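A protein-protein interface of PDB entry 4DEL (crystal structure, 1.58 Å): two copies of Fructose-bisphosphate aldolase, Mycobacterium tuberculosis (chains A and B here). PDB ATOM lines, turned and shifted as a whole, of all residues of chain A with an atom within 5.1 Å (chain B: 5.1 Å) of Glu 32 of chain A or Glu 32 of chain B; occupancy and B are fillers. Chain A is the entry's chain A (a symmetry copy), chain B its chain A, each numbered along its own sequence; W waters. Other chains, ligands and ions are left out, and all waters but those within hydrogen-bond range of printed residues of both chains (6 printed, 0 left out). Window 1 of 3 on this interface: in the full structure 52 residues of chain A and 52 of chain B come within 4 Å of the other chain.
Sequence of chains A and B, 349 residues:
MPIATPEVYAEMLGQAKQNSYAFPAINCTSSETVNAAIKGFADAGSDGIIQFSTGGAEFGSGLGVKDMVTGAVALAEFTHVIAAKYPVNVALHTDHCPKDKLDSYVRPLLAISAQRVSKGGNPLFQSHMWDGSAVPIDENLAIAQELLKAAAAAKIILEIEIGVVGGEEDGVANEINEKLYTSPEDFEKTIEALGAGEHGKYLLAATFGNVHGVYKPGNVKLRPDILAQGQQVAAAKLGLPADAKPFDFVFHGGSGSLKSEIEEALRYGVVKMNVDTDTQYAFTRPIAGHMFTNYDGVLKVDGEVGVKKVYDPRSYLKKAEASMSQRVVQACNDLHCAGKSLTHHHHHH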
ATOM      1  N   SER A  30      20.952  27.113 -25.084  1.00  0.00           N
ATOM      2  CA  SER A  30      19.843  26.305 -25.586  1.00  0.00           C
ATOM      3  C   SER A  30      18.472  26.782 -25.109  1.00  0.00           C
ATOM      4  O   SER A  30      18.363  27.611 -24.187  1.00  0.00           O
ATOM      5  CB  SER A  30      20.026  24.865 -25.090  1.00  0.00           C
ATOM      6  OG  SER A  30      19.841  24.811 -23.673  1.00  0.00           O
ATOM      7  N   SER A  31      17.418  26.216 -25.696  1.00  0.00           N
ATOM      8  CA  SER A  31      16.084  26.462 -25.200  1.00  0.00           C
ATOM      9  C   SER A  31      15.957  26.041 -23.738  1.00  0.00           C
ATOM     10  O   SER A  31      15.347  26.765 -22.928  1.00  0.00           O
ATOM     11  CB  SER A  31      15.038  25.737 -26.058  1.00  0.00           C
ATOM     12  OG  SER A  31      15.420  24.375 -26.261  1.00  0.00           O
ATOM     13  N   GLU A  32      16.521  24.877 -23.382  1.00  0.00           N
ATOM     14  CA  GLU A  32      16.362  24.363 -22.007  1.00  0.00           C
ATOM     15  C   GLU A  32      17.065  25.255 -20.986  1.00  0.00           C
ATOM     16  O   GLU A  32      16.514  25.508 -19.904  1.00  0.00           O
ATOM     17  CB  GLU A  32      16.914  22.940 -21.867  1.00  0.00           C
ATOM     18  CG  GLU A  32      16.145  21.902 -22.672  1.00  0.00           C
ATOM     19  CD  GLU A  32      16.829  21.589 -24.000  1.00  0.00           C
ATOM     20  OE1 GLU A  32      17.526  22.455 -24.595  1.00  0.00           O
ATOM     21  OE2 GLU A  32      16.678  20.431 -24.434  1.00  0.00           O
ATOM     22  N   THR A  33      18.258  25.735 -21.334  1.00  0.00           N
ATOM     23  CA  THR A  33      19.049  26.557 -20.400  1.00  0.00           C
ATOM     24  C   THR A  33      18.452  27.974 -20.276  1.00  0.00           C
ATOM     25  O   THR A  33      18.322  28.509 -19.159  1.00  0.00           O
ATOM     26  CB  THR A  33      20.567  26.549 -20.719  1.00  0.00           C
ATOM     27  OG1 THR A  33      20.776  26.895 -22.089  1.00  0.00           O
ATOM     28  CG2 THR A  33      21.181  25.140 -20.452  1.00  0.00           C
ATOM     29  N   VAL A  34      18.013  28.547 -21.395  1.00  0.00           N
ATOM     30  CA  VAL A  34      17.213  29.798 -21.322  1.00  0.00           C
ATOM     31  C   VAL A  34      15.988  29.628 -20.415  1.00  0.00           C
ATOM     32  O   VAL A  34      15.751  30.448 -19.509  1.00  0.00           O
ATOM     33  CB  VAL A  34      16.778  30.269 -22.733  1.00  0.00           C
ATOM     34  CG1 VAL A  34      15.718  31.386 -22.645  1.00  0.00           C
ATOM     35  CG2 VAL A  34      17.985  30.728 -23.515  1.00  0.00           C
ATOM     36  N   ASN A  35      15.205  28.572 -20.642  1.00  0.00           N
ATOM     37  CA  ASN A  35      14.032  28.327 -19.819  1.00  0.00           C
ATOM     38  C   ASN A  35      14.378  28.191 -18.333  1.00  0.00           C
ATOM     39  O   ASN A  35      13.678  28.729 -17.466  1.00  0.00           O
ATOM     40  CB  ASN A  35      13.279  27.088 -20.318  1.00  0.00           C
ATOM     41  CG  ASN A  35      12.415  27.394 -21.529  1.00  0.00           C
ATOM     42  OD1 ASN A  35      12.012  28.547 -21.743  1.00  0.00           O
ATOM     43  ND2 ASN A  35      12.130  26.371 -22.336  1.00  0.00           N
ATOM     44  N   ALA A  36      15.473  27.487 -18.046  1.00  0.00           N
ATOM     45  CA  ALA A  36      15.911  27.295 -16.659  1.00  0.00           C
ATOM     46  C   ALA A  36      16.292  28.615 -16.014  1.00  0.00           C
ATOM     47  O   ALA A  36      15.918  28.883 -14.858  1.00  0.00           O
ATOM     48  CB  ALA A  36      17.098  26.308 -16.612  1.00  0.00           C
ATOM     49  N   ALA A  37      17.037  29.439 -16.755  1.00  0.00           N
ATOM     50  CA  ALA A  37      17.455  30.746 -16.238  1.00  0.00           C
ATOM     51  C   ALA A  37      16.259  31.649 -15.928  1.00  0.00           C
ATOM     52  O   ALA A  37      16.142  32.183 -14.806  1.00  0.00           O
ATOM     53  CB  ALA A  37      18.425  31.414 -17.173  1.00  0.00           C
ATOM     54  N   PHE A  59      27.344  26.906 -30.669  1.00  0.00           N
ATOM     55  CA  PHE A  59      26.616  25.688 -30.290  1.00  0.00           C
ATOM     56  C   PHE A  59      25.117  25.816 -30.610  1.00  0.00           C
ATOM     57  O   PHE A  59      24.498  24.890 -31.148  1.00  0.00           O
ATOM     58  CB  PHE A  59      26.830  25.382 -28.806  1.00  0.00           C
ATOM     59  CG  PHE A  59      25.980  24.247 -28.300  1.00  0.00           C
ATOM     60  CD1 PHE A  59      26.378  22.924 -28.488  1.00  0.00           C
ATOM     61  CD2 PHE A  59      24.778  24.509 -27.651  1.00  0.00           C
ATOM     62  CE1 PHE A  59      25.573  21.871 -28.023  1.00  0.00           C
ATOM     63  CE2 PHE A  59      23.973  23.477 -27.174  1.00  0.00           C
ATOM     64  CZ  PHE A  59      24.378  22.146 -27.367  1.00  0.00           C
ATOM     65  N   PHE A 283      22.887  21.944 -14.039  1.00  0.00           N
ATOM     66  CA  PHE A 283      22.084  21.404 -15.139  1.00  0.00           C
ATOM     67  C   PHE A 283      22.438  19.921 -15.349  1.00  0.00           C
ATOM     68  O   PHE A 283      21.569  19.069 -15.462  1.00  0.00           O
ATOM     69  CB  PHE A 283      22.370  22.216 -16.404  1.00  0.00           C
ATOM     70  CG  PHE A 283      21.461  21.895 -17.564  1.00  0.00           C
ATOM     71  CD1 PHE A 283      20.227  22.513 -17.682  1.00  0.00           C
ATOM     72  CD2 PHE A 283      21.865  20.986 -18.560  1.00  0.00           C
ATOM     73  CE1 PHE A 283      19.368  22.224 -18.778  1.00  0.00           C
ATOM     74  CE2 PHE A 283      21.012  20.711 -19.651  1.00  0.00           C
ATOM     75  CZ  PHE A 283      19.778  21.324 -19.756  1.00  0.00           C
ATOM     76  N   LEU A 317      15.822  16.075 -19.018  1.00  0.00           N
ATOM     77  CA  LEU A 317      16.017  17.522 -19.227  1.00  0.00           C
ATOM     78  C   LEU A 317      15.096  18.382 -18.379  1.00  0.00           C
ATOM     79  O   LEU A 317      15.469  19.499 -18.013  1.00  0.00           O
ATOM     80  CB  LEU A 317      15.944  17.902 -20.707  1.00  0.00           C
ATOM     81  CG  LEU A 317      17.130  17.344 -21.495  1.00  0.00           C
ATOM     82  CD1 LEU A 317      16.856  17.384 -22.999  1.00  0.00           C
ATOM     83  CD2 LEU A 317      18.425  18.088 -21.188  1.00  0.00           C
ATOM     84  N   GLU A 321      16.614  21.252 -16.040  1.00  0.00           N
ATOM     85  CA  GLU A 321      16.038  22.594 -15.988  1.00  0.00           C
ATOM     86  C   GLU A 321      15.787  23.025 -14.536  1.00  0.00           C
ATOM     87  O   GLU A 321      16.283  24.063 -14.094  1.00  0.00           O
ATOM     88  CB  GLU A 321      14.733  22.648 -16.789  1.00  0.00           C
ATOM     89  CG  GLU A 321      14.275  24.073 -17.122  1.00  0.00           C
ATOM     90  CD  GLU A 321      12.825  24.158 -17.590  1.00  0.00           C
ATOM     91  OE1 GLU A 321      12.076  25.009 -17.054  1.00  0.00           O
ATOM     92  OE2 GLU A 321      12.449  23.393 -18.503  1.00  0.00           O
ATOM     93  N   SER B  30      13.225  20.932 -28.624  1.00  0.00           N
ATOM     94  CA  SER B  30      14.288  21.831 -28.180  1.00  0.00           C
ATOM     95  C   SER B  30      15.129  22.396 -29.323  1.00  0.00           C
ATOM     96  O   SER B  30      15.058  21.924 -30.472  1.00  0.00           O
ATOM     97  CB  SER B  30      15.232  21.049 -27.259  1.00  0.00           C
ATOM     98  OG  SER B  30      15.944  20.064 -28.013  1.00  0.00           O
ATOM     99  N   SER B  31      15.975  23.375 -28.999  1.00  0.00           N
ATOM    100  CA  SER B  31      16.939  23.857 -29.960  1.00  0.00           C
ATOM    101  C   SER B  31      17.851  22.729 -30.434  1.00  0.00           C
ATOM    102  O   SER B  31      18.147  22.627 -31.640  1.00  0.00           O
ATOM    103  CB  SER B  31      17.770  25.007 -29.373  1.00  0.00           C
ATOM    104  OG  SER B  31      18.256  24.656 -28.076  1.00  0.00           O
ATOM    105  N   GLU B  32      18.311  21.879 -29.503  1.00  0.00           N
ATOM    106  CA  GLU B  32      19.269  20.818 -29.874  1.00  0.00           C
ATOM    107  C   GLU B  32      18.637  19.786 -30.806  1.00  0.00           C
ATOM    108  O   GLU B  32      19.283  19.344 -31.767  1.00  0.00           O
ATOM    109  CB  GLU B  32      19.809  20.087 -28.639  1.00  0.00           C
ATOM    110  CG  GLU B  32      20.660  20.964 -27.732  1.00  0.00           C
ATOM    111  CD  GLU B  32      19.861  21.502 -26.547  1.00  0.00           C
ATOM    112  OE1 GLU B  32      18.621  21.708 -26.637  1.00  0.00           O
ATOM    113  OE2 GLU B  32      20.503  21.694 -25.497  1.00  0.00           O
ATOM    114  N   THR B  33      17.384  19.422 -30.532  1.00  0.00           N
ATOM    115  CA  THR B  33      16.700  18.389 -31.332  1.00  0.00           C
ATOM    116  C   THR B  33      16.297  18.944 -32.713  1.00  0.00           C
ATOM    117  O   THR B  33      16.495  18.274 -33.745  1.00  0.00           O
ATOM    118  CB  THR B  33      15.533  17.707 -30.572  1.00  0.00           C
ATOM    119  OG1 THR B  33      14.644  18.700 -30.056  1.00  0.00           O
ATOM    120  CG2 THR B  33      16.071  16.844 -29.389  1.00  0.00           C
ATOM    121  N   VAL B  34      15.815  20.185 -32.752  1.00  0.00           N
ATOM    122  CA  VAL B  34      15.634  20.868 -34.060  1.00  0.00           C
ATOM    123  C   VAL B  34      16.936  20.885 -34.868  1.00  0.00           C
ATOM    124  O   VAL B  34      16.953  20.501 -36.052  1.00  0.00           O
ATOM    125  CB  VAL B  34      15.098  22.310 -33.869  1.00  0.00           C
ATOM    126  CG1 VAL B  34      15.183  23.113 -35.183  1.00  0.00           C
ATOM    127  CG2 VAL B  34      13.680  22.266 -33.352  1.00  0.00           C
ATOM    128  N   ASN B  35      18.032  21.324 -34.248  1.00  0.00           N
ATOM    129  CA  ASN B  35      19.312  21.359 -34.937  1.00  0.00           C
ATOM    130  C   ASN B  35      19.734  19.981 -35.457  1.00  0.00           C
ATOM    131  O   ASN B  35      20.227  19.852 -36.585  1.00  0.00           O
ATOM    132  CB  ASN B  35      20.394  21.951 -34.025  1.00  0.00           C
ATOM    133  CG  ASN B  35      20.332  23.468 -33.977  1.00  0.00           C
ATOM    134  OD1 ASN B  35      19.824  24.110 -34.909  1.00  0.00           O
ATOM    135  ND2 ASN B  35      20.839  24.054 -32.891  1.00  0.00           N
ATOM    136  N   ALA B  36      19.519  18.952 -34.638  1.00  0.00           N
ATOM    137  CA  ALA B  36      19.873  17.583 -35.028  1.00  0.00           C
ATOM    138  C   ALA B  36      19.056  17.122 -36.222  1.00  0.00           C
ATOM    139  O   ALA B  36      19.601  16.518 -37.163  1.00  0.00           O
ATOM    140  CB  ALA B  36      19.673  16.625 -33.834  1.00  0.00           C
ATOM    141  N   ALA B  37      17.751  17.402 -36.185  1.00  0.00           N
ATOM    142  CA  ALA B  37      16.866  17.014 -37.289  1.00  0.00           C
ATOM    143  C   ALA B  37      17.263  17.688 -38.605  1.00  0.00           C
ATOM    144  O   ALA B  37      17.454  17.006 -39.633  1.00  0.00           O
ATOM    145  CB  ALA B  37      15.426  17.274 -36.946  1.00  0.00           C
ATOM    146  N   PHE B  59       6.764  21.276 -23.126  1.00  0.00           N
ATOM    147  CA  PHE B  59       8.157  21.184 -22.670  1.00  0.00           C
ATOM    148  C   PHE B  59       8.989  22.368 -23.188  1.00  0.00           C
ATOM    149  O   PHE B  59       9.771  22.972 -22.444  1.00  0.00           O
ATOM    150  CB  PHE B  59       8.772  19.854 -23.110  1.00  0.00           C
ATOM    151  CG  PHE B  59      10.248  19.755 -22.829  1.00  0.00           C
ATOM    152  CD1 PHE B  59      10.707  19.390 -21.563  1.00  0.00           C
ATOM    153  CD2 PHE B  59      11.171  20.044 -23.829  1.00  0.00           C
ATOM    154  CE1 PHE B  59      12.086  19.312 -21.307  1.00  0.00           C
ATOM    155  CE2 PHE B  59      12.542  19.960 -23.594  1.00  0.00           C
ATOM    156  CZ  PHE B  59      12.999  19.594 -22.318  1.00  0.00           C
ATOM    157  N   PHE B 283      19.337  10.244 -29.551  1.00  0.00           N
ATOM    158  CA  PHE B 283      19.793  11.468 -28.887  1.00  0.00           C
ATOM    159  C   PHE B 283      20.370  11.115 -27.505  1.00  0.00           C
ATOM    160  O   PHE B 283      21.446  11.559 -27.132  1.00  0.00           O
ATOM    161  CB  PHE B 283      18.608  12.427 -28.752  1.00  0.00           C
ATOM    162  CG  PHE B 283      18.980  13.806 -28.267  1.00  0.00           C
ATOM    163  CD1 PHE B 283      19.410  14.773 -29.161  1.00  0.00           C
ATOM    164  CD2 PHE B 283      18.868  14.140 -26.905  1.00  0.00           C
ATOM    165  CE1 PHE B 283      19.752  16.079 -28.713  1.00  0.00           C
ATOM    166  CE2 PHE B 283      19.200  15.442 -26.469  1.00  0.00           C
ATOM    167  CZ  PHE B 283      19.638  16.398 -27.364  1.00  0.00           C
ATOM    168  N   LEU B 317      25.857  17.186 -25.256  1.00  0.00           N
ATOM    169  CA  LEU B 317      24.758  17.519 -26.183  1.00  0.00           C
ATOM    170  C   LEU B 317      25.201  17.603 -27.634  1.00  0.00           C
ATOM    171  O   LEU B 317      24.404  17.320 -28.532  1.00  0.00           O
ATOM    172  CB  LEU B 317      24.001  18.775 -25.747  1.00  0.00           C
ATOM    173  CG  LEU B 317      23.216  18.544 -24.455  1.00  0.00           C
ATOM    174  CD1 LEU B 317      22.796  19.871 -23.824  1.00  0.00           C
ATOM    175  CD2 LEU B 317      21.988  17.668 -24.679  1.00  0.00           C
ATOM    176  N   GLU B 321      23.312  15.463 -30.439  1.00  0.00           N
ATOM    177  CA  GLU B 321      22.912  16.045 -31.718  1.00  0.00           C
ATOM    178  C   GLU B 321      23.388  15.171 -32.888  1.00  0.00           C
ATOM    179  O   GLU B 321      22.584  14.739 -33.717  1.00  0.00           O
ATOM    180  CB  GLU B 321      23.469  17.465 -31.858  1.00  0.00           C
ATOM    181  CG  GLU B 321      22.787  18.286 -32.959  1.00  0.00           C
ATOM    182  CD  GLU B 321      23.554  19.547 -33.349  1.00  0.00           C
ATOM    183  OE1 GLU B 321      23.761  19.764 -34.566  1.00  0.00           O
ATOM    184  OE2 GLU B 321      23.926  20.321 -32.442  1.00  0.00           O
HETATM  185  O   HOH W   1      20.412  22.403 -22.822  1.00  0.00           O
HETATM  186  O   HOH W   2      25.600  22.307 -31.774  1.00  0.00           O
HETATM  187  O   HOH W   3      10.342  22.259 -19.715  1.00  0.00           O
HETATM  188  O   HOH W   4      17.350  18.579 -26.379  1.00  0.00           O
HETATM  189  O   HOH W   5      22.234  23.289 -30.391  1.00  0.00           O
HETATM  190  O   HOH W   6      12.606  23.450 -22.483  1.00  0.00           O
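Of the printed residues of chain A, Glu 32 of chain B touches Ser 30, Glu 32 and Phe 59. Of the printed residues of chain B, Ser 30 of chain A touches Ser 31 (3.4 Å) and Glu 32 (3.2 Å). Of the printed residues of chain B, Leu 317 of chain A touches Phe 59 (3.8 Å). Of the printed residues of chain A, Leu 317 of chain B touches Phe 59 (3.8 Å). Glu 321 of chain B touches none of the printed residues of chain A. Val 34 of chain A touches none of the printed residues of chain B.
The backbone NH (N) of Ser 31 of chain B is in hydrogen-bond range of the side-chain hydroxyl (OG) of Ser 31 of chain A (3.0 Å). The side-chain carboxylate (OE1) of Glu 32 of chain A sits close to the side-chain carboxylate (OE1) of Glu 32 of chain B.
Ser 30 of chain A touches Ser 31 of chain B (CA to OG, 3.4 Å). CB of Ser 30 of chain A touches OE2 of Glu 32 of chain B (3.2 Å). CA of Ser 30 of chain B touches OG of Ser 31 of chain A (3.4 Å). Glu 32 of chain A touches Ser 30 of chain B (OE2 to CB, 3.2 Å). Glu 32 of chain A touches Phe 59 of chain B. Glu 32 of chain B touches Phe 59 of chain A (CG to CZ, 3.9 Å). Phe 59 of chain A touches Leu 317 of chain B. CB of Leu 317 of chain A touches CZ of Phe 59 of chain B, at 3.8 Å.
The side-chain hydroxyl (OG1) of Thr 33 of chain B lies within hydrogen-bond range of the side-chain hydroxyl (OG) of Ser 30 of chain B (2.8 Å). OE1 of Glu 32 of chain B is in hydrogen-bond range of OG of Ser 31 of chain B. The side-chain amide nitrogen (ND2) of Asn 35 of chain B is in hydrogen-bond range of the backbone carbonyl oxygen (O) of Ser 31 of chain B (3.3 Å). The backbone NH (N) of Glu 32 of chain A sits close to the side-chain hydroxyl (OG) of Ser 30 of chain A (3.3 Å). The side-chain hydroxyl of Ser 31 of chain A sits at hydrogen-bond distance from the side-chain carboxylate of Glu 32 of chain A. The backbone carbonyl oxygen (O) of Ser 31 of chain A is in hydrogen-bond range of the side-chain amide nitrogen (ND2) of Asn 35 of chain A.
Water W4 lies within hydrogen-bond range of the side-chain hydroxyl (OG) of Ser 30 of chain B (2.6 Å), the side-chain carboxylate (OE2) of Glu 32 of chain A (2.8 Å) and the side-chain carboxylate (OE1) of Glu 32 of chain B (3.4 Å). Water W1 lies within hydrogen-bond range of OG of Ser 30 of chain A (2.6 Å), OE2 of Glu 32 of chain B (2.8 Å) and OE1 of Glu 32 of chain A (3.4 Å). Water W2 lies within hydrogen-bond range of the side-chain carboxylate of Glu 321 of chain B and the backbone carbonyl oxygen of Phe 59 of chain A. Water W3 bridges the side-chain carboxylate (OE2) of Glu 321 of chain A and the backbone carbonyl oxygen (O) of Phe 59 of chain B. Water W6 lies within hydrogen-bond range of the backbone carbonyl oxygen of Phe 59 of chain B and the side-chain amide nitrogen of Asn 35 of chain A. Water W5 bridges the backbone carbonyl oxygen of Phe 59 of chain A (2.9 Å) and the side-chain amide nitrogen of Asn 35 of chain B (3.0 Å).
Of the 12 printed residues of chain B, 5 touch a printed residue of chain A. Hydrophobic or aromatic side chains of chain B within 4 Å of the printed part of chain A: Phe 59 and Leu 317. Of the 12 printed residues of chain A, 5 touch a printed residue of chain B. Printed residues of chain A that touch a printed residue of chain B: Ser 30, Ser 31, Glu 32, Phe 59 and Leu 317. Hydrophobic or aromatic side chains of chain A within 4 Å of the printed part of chain B: Phe 59 and Leu 317. Among the printed residues, 10 pairs touch across the chains. Among the printed residues, no Asp or Glu carboxylate lies within 4 Å of a Lys or Arg side-chain nitrogen of the other chain.
Ser 30 of chain A touches Ser 31 of chain B, and with the chains exchanged Ser 31 of chain A touches Ser 30 of chain B. Ser 31 of chain B touches its own counterpart, Ser 31 of chain A. Glu 32 of chain B touches its own counterpart, Glu 32 of chain A. Glu 32 of chain A touches Phe 59 of chain B, and with the chains exchanged Phe 59 of chain A touches Glu 32 of chain B. Of the 10 pairs that touch across the chains among the printed residues, 10 have their exchanged pair printed and touching as well.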
